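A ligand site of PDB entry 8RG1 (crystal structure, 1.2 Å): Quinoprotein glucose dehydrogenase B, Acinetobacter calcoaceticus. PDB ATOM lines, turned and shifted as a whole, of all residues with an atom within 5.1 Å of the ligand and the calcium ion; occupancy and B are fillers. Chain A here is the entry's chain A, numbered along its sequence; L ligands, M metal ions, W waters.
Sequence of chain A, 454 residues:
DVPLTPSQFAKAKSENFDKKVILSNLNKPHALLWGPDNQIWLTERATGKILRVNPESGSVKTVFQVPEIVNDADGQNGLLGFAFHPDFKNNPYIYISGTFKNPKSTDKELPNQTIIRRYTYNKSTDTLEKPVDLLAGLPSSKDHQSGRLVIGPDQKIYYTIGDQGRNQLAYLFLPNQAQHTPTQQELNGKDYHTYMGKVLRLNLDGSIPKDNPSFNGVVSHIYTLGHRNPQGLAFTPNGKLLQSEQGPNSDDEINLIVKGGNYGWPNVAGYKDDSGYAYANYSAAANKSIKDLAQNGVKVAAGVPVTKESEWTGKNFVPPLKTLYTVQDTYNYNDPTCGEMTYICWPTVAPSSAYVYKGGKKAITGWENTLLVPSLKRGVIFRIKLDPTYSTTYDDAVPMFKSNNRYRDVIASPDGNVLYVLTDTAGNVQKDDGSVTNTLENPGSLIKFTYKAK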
ATOM      1  N   GLN A  76       5.113 -29.263  24.107  1.00  0.00           N
ATOM      2  CA  GLN A  76       3.896 -29.183  23.321  1.00  0.00           C
ATOM      3  C   GLN A  76       3.365 -30.568  22.971  1.00  0.00           C
ATOM      4  O   GLN A  76       2.542 -30.712  22.074  1.00  0.00           O
ATOM      5  CB  GLN A  76       4.193 -28.385  22.048  1.00  0.00           C
ATOM      6  CG  GLN A  76       4.498 -26.921  22.336  1.00  0.00           C
ATOM      7  CD  GLN A  76       5.100 -26.098  21.155  1.00  0.00           C
ATOM      8  OE1 GLN A  76       5.278 -26.558  20.007  1.00  0.00           O
ATOM      9  NE2 GLN A  76       5.455 -24.863  21.469  1.00  0.00           N
ATOM     10  N   HIS A 144       7.010 -28.253  18.437  1.00  0.00           N
ATOM     11  CA  HIS A 144       6.528 -28.268  17.049  1.00  0.00           C
ATOM     12  C   HIS A 144       6.009 -29.650  16.680  1.00  0.00           C
ATOM     13  O   HIS A 144       6.449 -30.286  15.723  1.00  0.00           O
ATOM     14  CB  HIS A 144       7.602 -27.844  16.049  1.00  0.00           C
ATOM     15  CG  HIS A 144       8.141 -26.494  16.283  1.00  0.00           C
ATOM     16  ND1 HIS A 144       9.198 -25.995  15.552  1.00  0.00           N
ATOM     17  CD2 HIS A 144       7.793 -25.523  17.158  1.00  0.00           C
ATOM     18  CE1 HIS A 144       9.499 -24.791  15.986  1.00  0.00           C
ATOM     19  NE2 HIS A 144       8.655 -24.476  16.951  1.00  0.00           N
ATOM     20  N   ARG A 228       6.962 -26.133   9.153  1.00  0.00           N
ATOM     21  CA  ARG A 228       7.619 -25.920  10.432  1.00  0.00           C
ATOM     22  C   ARG A 228       6.694 -26.383  11.530  1.00  0.00           C
ATOM     23  O   ARG A 228       6.936 -27.428  12.127  1.00  0.00           O
ATOM     24  CB  ARG A 228       7.954 -24.446  10.619  1.00  0.00           C
ATOM     25  CG  ARG A 228       8.627 -24.162  11.900  1.00  0.00           C
ATOM     26  CD  ARG A 228       9.053 -22.715  11.923  1.00  0.00           C
ATOM     27  NE  ARG A 228       9.704 -22.333  13.168  1.00  0.00           N
ATOM     28  CZ  ARG A 228       9.053 -22.040  14.282  1.00  0.00           C
ATOM     29  NH1 ARG A 228       7.740 -22.119  14.356  1.00  0.00           N
ATOM     30  NH2 ARG A 228       9.752 -21.694  15.363  1.00  0.00           N
ATOM     31  N   ASN A 229       5.646 -25.642  11.828  1.00  0.00           N
ATOM     32  CA  ASN A 229       4.703 -26.032  12.879  1.00  0.00           C
ATOM     33  C   ASN A 229       3.297 -25.762  12.403  1.00  0.00           C
ATOM     34  O   ASN A 229       2.679 -24.767  12.767  1.00  0.00           O
ATOM     35  CB  ASN A 229       4.996 -25.336  14.204  1.00  0.00           C
ATOM     36  CG  ASN A 229       4.222 -25.919  15.320  1.00  0.00           C
ATOM     37  OD1 ASN A 229       3.691 -27.004  15.179  1.00  0.00           O
ATOM     38  ND2 ASN A 229       4.149 -25.220  16.432  1.00  0.00           N
ATOM     39  N   GLN A 231      -0.136 -25.904  12.730  1.00  0.00           N
ATOM     40  CA  GLN A 231      -1.113 -26.203  13.773  1.00  0.00           C
ATOM     41  C   GLN A 231      -2.544 -26.187  13.275  1.00  0.00           C
ATOM     42  O   GLN A 231      -3.423 -26.737  13.948  1.00  0.00           O
ATOM     43  CB  GLN A 231      -1.040 -25.191  14.926  1.00  0.00           C
ATOM     44  CG  GLN A 231       0.280 -25.114  15.649  1.00  0.00           C
ATOM     45  CD  GLN A 231       0.286 -26.027  16.846  1.00  0.00           C
ATOM     46  OE1 GLN A 231      -0.257 -27.130  16.795  1.00  0.00           O
ATOM     47  NE2 GLN A 231       0.893 -25.571  17.939  1.00  0.00           N
ATOM     48  N   GLN A 246       3.039 -21.892  12.104  1.00  0.00           N
ATOM     49  CA  GLN A 246       3.887 -20.974  12.832  1.00  0.00           C
ATOM     50  C   GLN A 246       5.248 -20.931  12.179  1.00  0.00           C
ATOM     51  O   GLN A 246       5.910 -21.960  12.021  1.00  0.00           O
ATOM     52  CB  GLN A 246       4.032 -21.438  14.278  1.00  0.00           C
ATOM     53  CG  GLN A 246       2.728 -21.466  14.994  1.00  0.00           C
ATOM     54  CD  GLN A 246       2.866 -21.633  16.456  1.00  0.00           C
ATOM     55  OE1 GLN A 246       3.957 -21.813  16.970  1.00  0.00           O
ATOM     56  NE2 GLN A 246       1.746 -21.624  17.146  1.00  0.00           N
ATOM     57  N   GLY A 247       5.691 -19.737  11.872  1.00  0.00           N
ATOM     58  CA  GLY A 247       7.037 -19.466  11.425  1.00  0.00           C
ATOM     59  C   GLY A 247       7.944 -19.159  12.593  1.00  0.00           C
ATOM     60  O   GLY A 247       7.553 -19.223  13.757  1.00  0.00           O
ATOM     61  N   PRO A 248       9.194 -18.828  12.290  1.00  0.00           N
ATOM     62  CA  PRO A 248      10.201 -18.562  13.324  1.00  0.00           C
ATOM     63  C   PRO A 248      10.000 -17.175  13.917  1.00  0.00           C
ATOM     64  O   PRO A 248       8.995 -16.935  14.592  1.00  0.00           O
ATOM     65  CB  PRO A 248      11.523 -18.744  12.580  1.00  0.00           C
ATOM     66  CG  PRO A 248      11.193 -18.356  11.175  1.00  0.00           C
ATOM     67  CD  PRO A 248       9.780 -18.835  10.940  1.00  0.00           C
ATOM     68  N   ASN A 249      10.883 -16.205  13.645  1.00  0.00           N
ATOM     69  CA  ASN A 249      10.625 -14.879  14.154  1.00  0.00           C
ATOM     70  C   ASN A 249       9.696 -14.081  13.244  1.00  0.00           C
ATOM     71  O   ASN A 249       9.370 -12.928  13.547  1.00  0.00           O
ATOM     72  CB  ASN A 249      11.890 -14.020  14.226  1.00  0.00           C
ATOM     73  CG  ASN A 249      13.006 -14.583  15.091  1.00  0.00           C
ATOM     74  OD1 ASN A 249      13.063 -15.745  15.429  1.00  0.00           O
ATOM     75  ND2 ASN A 249      13.950 -13.705  15.415  1.00  0.00           N
ATOM     76  N   ASP A 252       4.736 -16.424   9.956  1.00  0.00           N
ATOM     77  CA  ASP A 252       3.624 -17.357  10.102  1.00  0.00           C
ATOM     78  C   ASP A 252       2.864 -17.358   8.780  1.00  0.00           C
ATOM     79  O   ASP A 252       2.859 -16.370   8.056  1.00  0.00           O
ATOM     80  CB  ASP A 252       2.666 -16.920  11.204  1.00  0.00           C
ATOM     81  CG  ASP A 252       3.290 -16.947  12.588  1.00  0.00           C
ATOM     82  OD1 ASP A 252       4.208 -17.755  12.818  1.00  0.00           O
ATOM     83  OD2 ASP A 252       2.813 -16.203  13.443  1.00  0.00           O
ATOM     84  N   TYR A 343      10.618 -11.027  21.925  1.00  0.00           N
ATOM     85  CA  TYR A 343       9.978 -11.877  20.932  1.00  0.00           C
ATOM     86  C   TYR A 343       8.471 -11.669  20.823  1.00  0.00           C
ATOM     87  O   TYR A 343       7.874 -12.175  19.866  1.00  0.00           O
ATOM     88  CB  TYR A 343      10.338 -13.358  21.177  1.00  0.00           C
ATOM     89  CG  TYR A 343       9.398 -14.171  22.051  1.00  0.00           C
ATOM     90  CD1 TYR A 343       9.183 -13.853  23.383  1.00  0.00           C
ATOM     91  CD2 TYR A 343       8.774 -15.308  21.543  1.00  0.00           C
ATOM     92  CE1 TYR A 343       8.345 -14.630  24.182  1.00  0.00           C
ATOM     93  CE2 TYR A 343       7.939 -16.077  22.323  1.00  0.00           C
ATOM     94  CZ  TYR A 343       7.725 -15.738  23.643  1.00  0.00           C
ATOM     95  OH  TYR A 343       6.891 -16.506  24.424  1.00  0.00           O
ATOM     96  N   ILE A 344       7.852 -10.927  21.729  1.00  0.00           N
ATOM     97  CA  ILE A 344       6.430 -10.605  21.556  1.00  0.00           C
ATOM     98  C   ILE A 344       6.222  -9.479  20.556  1.00  0.00           C
ATOM     99  O   ILE A 344       5.113  -9.352  20.013  1.00  0.00           O
ATOM    100  CB  ILE A 344       5.751 -10.349  22.905  1.00  0.00           C
ATOM    101  CG1 ILE A 344       6.177 -11.417  23.918  1.00  0.00           C
ATOM    102  CG2 ILE A 344       4.242 -10.360  22.760  1.00  0.00           C
ATOM    103  CD1 ILE A 344       5.969 -12.815  23.466  1.00  0.00           C
ATOM    104  N   TRP A 346       8.077  -9.608  17.907  1.00  0.00           N
ATOM    105  CA  TRP A 346       8.435 -10.259  16.647  1.00  0.00           C
ATOM    106  C   TRP A 346       7.235 -10.209  15.703  1.00  0.00           C
ATOM    107  O   TRP A 346       6.092 -10.340  16.166  1.00  0.00           O
ATOM    108  CB  TRP A 346       8.861 -11.711  16.783  1.00  0.00           C
ATOM    109  CG  TRP A 346      10.222 -11.942  17.347  1.00  0.00           C
ATOM    110  CD1 TRP A 346      11.186 -11.008  17.622  1.00  0.00           C
ATOM    111  CD2 TRP A 346      10.754 -13.209  17.714  1.00  0.00           C
ATOM    112  NE1 TRP A 346      12.272 -11.630  18.162  1.00  0.00           N
ATOM    113  CE2 TRP A 346      12.056 -12.978  18.237  1.00  0.00           C
ATOM    114  CE3 TRP A 346      10.273 -14.505  17.685  1.00  0.00           C
ATOM    115  CZ2 TRP A 346      12.869 -14.011  18.689  1.00  0.00           C
ATOM    116  CZ3 TRP A 346      11.063 -15.538  18.143  1.00  0.00           C
ATOM    117  CH2 TRP A 346      12.358 -15.281  18.655  1.00  0.00           C
ATOM    118  N   THR A 348       5.163 -11.903  14.120  1.00  0.00           N
ATOM    119  CA  THR A 348       4.426 -13.131  14.041  1.00  0.00           C
ATOM    120  C   THR A 348       3.202 -13.034  14.932  1.00  0.00           C
ATOM    121  O   THR A 348       3.062 -12.108  15.746  1.00  0.00           O
ATOM    122  CB  THR A 348       5.268 -14.290  14.540  1.00  0.00           C
ATOM    123  OG1 THR A 348       5.675 -14.006  15.873  1.00  0.00           O
ATOM    124  CG2 THR A 348       6.458 -14.522  13.657  1.00  0.00           C
ATOM    125  N   ALA A 350       1.794 -16.435  15.945  1.00  0.00           N
ATOM    126  CA  ALA A 350       1.724 -17.762  16.551  1.00  0.00           C
ATOM    127  C   ALA A 350       0.326 -18.355  16.389  1.00  0.00           C
ATOM    128  O   ALA A 350      -0.388 -18.585  17.367  1.00  0.00           O
ATOM    129  CB  ALA A 350       2.120 -17.728  18.022  1.00  0.00           C
ATOM    130  N   PRO A 351      -0.097 -18.631  15.158  1.00  0.00           N
ATOM    131  CA  PRO A 351      -1.421 -19.200  14.953  1.00  0.00           C
ATOM    132  C   PRO A 351      -1.484 -20.582  15.546  1.00  0.00           C
ATOM    133  O   PRO A 351      -0.559 -21.387  15.397  1.00  0.00           O
ATOM    134  CB  PRO A 351      -1.547 -19.280  13.433  1.00  0.00           C
ATOM    135  CG  PRO A 351      -0.143 -19.353  12.958  1.00  0.00           C
ATOM    136  CD  PRO A 351       0.642 -18.465  13.906  1.00  0.00           C
ATOM    137  N   LEU A 376      -1.978 -17.191  19.507  1.00  0.00           N
ATOM    138  CA  LEU A 376      -1.556 -17.426  20.868  1.00  0.00           C
ATOM    139  C   LEU A 376      -0.929 -16.163  21.447  1.00  0.00           C
ATOM    140  O   LEU A 376      -1.260 -15.731  22.541  1.00  0.00           O
ATOM    141  CB  LEU A 376      -0.537 -18.551  20.900  1.00  0.00           C
ATOM    142  CG  LEU A 376      -1.121 -19.898  20.513  1.00  0.00           C
ATOM    143  CD1 LEU A 376      -0.026 -20.878  20.191  1.00  0.00           C
ATOM    144  CD2 LEU A 376      -2.010 -20.448  21.611  1.00  0.00           C
ATOM    145  N   LYS A 377      -0.003 -15.570  20.713  1.00  0.00           N
ATOM    146  CA  LYS A 377       0.842 -14.536  21.282  1.00  0.00           C
ATOM    147  C   LYS A 377       0.139 -13.191  21.312  1.00  0.00           C
ATOM    148  O   LYS A 377       0.458 -12.359  22.157  1.00  0.00           O
ATOM    149  CB  LYS A 377       2.096 -14.423  20.406  1.00  0.00           C
ATOM    150  CG  LYS A 377       2.835 -13.162  20.590  1.00  0.00           C
ATOM    151  CD  LYS A 377       4.170 -13.298  19.960  1.00  0.00           C
ATOM    152  CE  LYS A 377       4.251 -12.482  18.734  1.00  0.00           C
ATOM    153  NZ  LYS A 377       5.619 -12.502  18.265  1.00  0.00           N
ATOM    154  N   ARG A 406      -4.222 -16.647  25.486  1.00  0.00           N
ATOM    155  CA  ARG A 406      -3.604 -17.369  24.388  1.00  0.00           C
ATOM    156  C   ARG A 406      -4.703 -18.231  23.785  1.00  0.00           C
ATOM    157  O   ARG A 406      -5.088 -19.232  24.373  1.00  0.00           O
ATOM    158  CB  ARG A 406      -2.459 -18.216  24.912  1.00  0.00           C
ATOM    159  CG  ARG A 406      -1.302 -17.407  25.411  1.00  0.00           C
ATOM    160  CD  ARG A 406      -0.308 -18.292  26.101  1.00  0.00           C
ATOM    161  NE  ARG A 406       0.225 -19.335  25.239  1.00  0.00           N
ATOM    162  CZ  ARG A 406       1.119 -19.152  24.283  1.00  0.00           C
ATOM    163  NH1 ARG A 406       1.656 -17.981  24.051  1.00  0.00           N
ATOM    164  NH2 ARG A 406       1.511 -20.197  23.562  1.00  0.00           N
ATOM    165  N   ARG A 408      -6.302 -20.900  21.607  1.00  0.00           N
ATOM    166  CA  ARG A 408      -5.745 -22.172  21.169  1.00  0.00           C
ATOM    167  C   ARG A 408      -6.567 -22.842  20.081  1.00  0.00           C
ATOM    168  O   ARG A 408      -6.021 -23.585  19.272  1.00  0.00           O
ATOM    169  CB  ARG A 408      -5.608 -23.095  22.374  1.00  0.00           C
ATOM    170  CG  ARG A 408      -5.204 -24.525  22.091  1.00  0.00           C
ATOM    171  CD  ARG A 408      -3.851 -24.630  21.434  1.00  0.00           C
ATOM    172  NE  ARG A 408      -2.785 -24.023  22.213  1.00  0.00           N
ATOM    173  CZ  ARG A 408      -1.520 -23.979  21.822  1.00  0.00           C
ATOM    174  NH1 ARG A 408      -1.144 -24.450  20.640  1.00  0.00           N
ATOM    175  NH2 ARG A 408      -0.614 -23.444  22.627  1.00  0.00           N
ATOM    176  N   ASN A 428       2.711 -16.756  27.800  1.00  0.00           N
ATOM    177  CA  ASN A 428       2.829 -15.332  27.619  1.00  0.00           C
ATOM    178  C   ASN A 428       1.862 -14.863  26.547  1.00  0.00           C
ATOM    179  O   ASN A 428       1.590 -15.553  25.576  1.00  0.00           O
ATOM    180  CB  ASN A 428       4.234 -14.977  27.166  1.00  0.00           C
ATOM    181  CG  ASN A 428       5.231 -15.216  28.241  1.00  0.00           C
ATOM    182  OD1 ASN A 428       4.919 -15.089  29.430  1.00  0.00           O
ATOM    183  ND2 ASN A 428       6.456 -15.573  27.855  1.00  0.00           N
HETATM  184  C1  LIG L   1       5.035 -18.281  20.466  1.00  0.00           C
HETATM  185  C2  LIG L   1       5.480 -17.087  19.924  1.00  0.00           C
HETATM  186  C3  LIG L   1       6.213 -17.169  18.756  1.00  0.00           C
HETATM  187  C4  LIG L   1       6.133 -19.466  18.679  1.00  0.00           C
HETATM  188  C5  LIG L   1       4.893 -20.671  20.501  1.00  0.00           C
HETATM  189  C6  LIG L   1       4.237 -22.282  21.961  1.00  0.00           C
HETATM  190  C7  LIG L   1       6.188 -20.813  22.754  1.00  0.00           C
HETATM  191  C8  LIG L   1       6.604 -20.663  17.890  1.00  0.00           C
HETATM  192  C9  LIG L   1       6.669 -15.907  18.047  1.00  0.00           C
HETATM  193  C10 LIG L   1       3.453 -22.375  20.839  1.00  0.00           C
HETATM  194  C11 LIG L   1       5.147 -21.220  21.759  1.00  0.00           C
HETATM  195  C12 LIG L   1       2.336 -23.299  20.495  1.00  0.00           C
HETATM  196  C13 LIG L   1       4.142 -18.155  21.680  1.00  0.00           C
HETATM  197  C14 LIG L   1       5.364 -19.506  19.861  1.00  0.00           C
HETATM  198  N1  LIG L   1       3.863 -21.400  19.962  1.00  0.00           N
HETATM  199  N2  LIG L   1       6.541 -18.310  18.157  1.00  0.00           N
HETATM  200  O1  LIG L   1       3.129 -18.824  21.711  1.00  0.00           O
HETATM  201  O2  LIG L   1       6.204 -21.431  23.834  1.00  0.00           O
HETATM  202  O3  LIG L   1       6.948 -19.881  22.428  1.00  0.00           O
HETATM  203  O4  LIG L   1       1.843 -23.953  21.427  1.00  0.00           O
HETATM  204  O5  LIG L   1       1.999 -23.377  19.295  1.00  0.00           O
HETATM  205  O6  LIG L   1       6.678 -21.768  18.482  1.00  0.00           O
HETATM  206  O7  LIG L   1       6.953 -20.458  16.673  1.00  0.00           O
HETATM  207  O8  LIG L   1       6.596 -14.850  18.677  1.00  0.00           O
HETATM  208  O9  LIG L   1       7.089 -16.078  16.879  1.00  0.00           O
HETATM  209  O10 LIG L   1       4.483 -17.360  22.602  1.00  0.00           O
HETATM  210 CA    CA M   1       7.452 -18.257  15.875  1.00  0.00          CA
HETATM  211  O   HOH W   1       8.032 -21.028  25.458  1.00  0.00           O
HETATM  212  O   HOH W   2       9.470 -18.780  16.919  1.00  0.00           O
HETATM  213  O   HOH W   3       5.154 -17.881  15.315  1.00  0.00           O
HETATM  214  O   HOH W   4       8.967 -22.652  18.857  1.00  0.00           O
HETATM  215  O   HOH W   5       3.605 -15.068  23.685  1.00  0.00           O
HETATM  216  O   HOH W   6       0.755 -26.639  22.782  1.00  0.00           O
HETATM  217  O   HOH W   7       3.866 -21.379  25.794  1.00  0.00           O
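Water W4 lies within hydrogen-bond range of an oxygen (O6) of the ligand (2.5 Å) and a ring nitrogen (NE2) of His 144 (2.7 Å). Water W5 bridges O10 of the ligand (2.7 Å) and O of Asn 428 (2.8 Å). Water W7 bridges an oxygen (O2) of the ligand (3.1 Å) and the guanidinium group of Arg 406 (3.5 Å). Water W6 lies within hydrogen-bond range of an oxygen (O4) of the ligand and the guanidinium group (NH2) of Arg 408.
Within 4 Å of the calcium ion: Gly 247 and Pro 248. The nearest printed residue that does not touch the calcium ion is Arg 228 (4.2 Å).
NZ of Lys 377 lies within salt-bridge range of O8 of the ligand, at 2.6 Å. O8 of the ligand lies close to OG1 of Thr 348, at 3.1 Å. An oxygen (O4) of the ligand is in salt-bridge range of the guanidinium group (NH2) of Arg 408, 2.8 Å away. O5 of the ligand sits at hydrogen-bond distance from NE2 of Gln 246 (2.8 Å). The side-chain amide nitrogen (NE2) of Gln 231 sits at hydrogen-bond distance from an oxygen (O5) of the ligand (2.8 Å). O1 of the ligand is in salt-bridge range of NH2 of Arg 406. NH1 of Arg 228 lies close to O7 of the ligand, 3.0 Å away. O10 of the ligand sits at hydrogen-bond distance from OH of Tyr 343 (3.1 Å).
The backbone carbonyl oxygen of Gly 247 lies close to the guanidinium group of Arg 228 (3.0 Å). OD1 of Asp 252 lies within hydrogen-bond range of N of Gly 247, 2.7 Å away. The side-chain amino group (NZ) of Lys 377 is in hydrogen-bond range of the backbone carbonyl oxygen (O) of Tyr 343 (2.8 Å). The guanidinium group (NH1) of Arg 228 is in hydrogen-bond range of the backbone carbonyl oxygen (O) of Gln 246, at 3.0 Å. The backbone carbonyl oxygen (O) of Asn 428 lies within hydrogen-bond range of the guanidinium group (NH1) of Arg 406 (2.9 Å). The side-chain amide oxygen (OE1) of Gln 76 sits at hydrogen-bond distance from the backbone NH (N) of His 144 (2.9 Å). NE2 of His 144 sits close to NH2 of Arg 228 (3.4 Å). N of Leu 376 lies within hydrogen-bond range of O of Ala 350, 3.0 Å away.
NE2 of Gln 76 touches C6 of the ligand, 2.9 Å away. His 144 touches the ligand. CE3 of Trp 346 touches O9 of the ligand, 3.6 Å away. Ala 350 touches the ligand. CD1 of Leu 376 touches O5 of the ligand (3.3 Å). Hydrophobic or aromatic side chains within 4 Å of the ligand: Tyr 343, Trp 346, Ala 350 and Leu 376. The nearest printed residue that does not touch the ligand is Asn 229 (4.03 Å).
O of Gly 247 is bound to the calcium ion (2.3 Å). Water W2 is bound to the calcium ion. O7 of the ligand binds the calcium ion, 2.4 Å away. Water W3 is bound to the calcium ion. The calcium ion is bound by the backbone carbonyl oxygen (O) of Pro 248. The calcium ion is bound by O9 of the ligand (2.4 Å). The calcium ion is bound by a nitrogen (N2) of the ligand. The calcium ion has seven donor atoms within binding distance.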
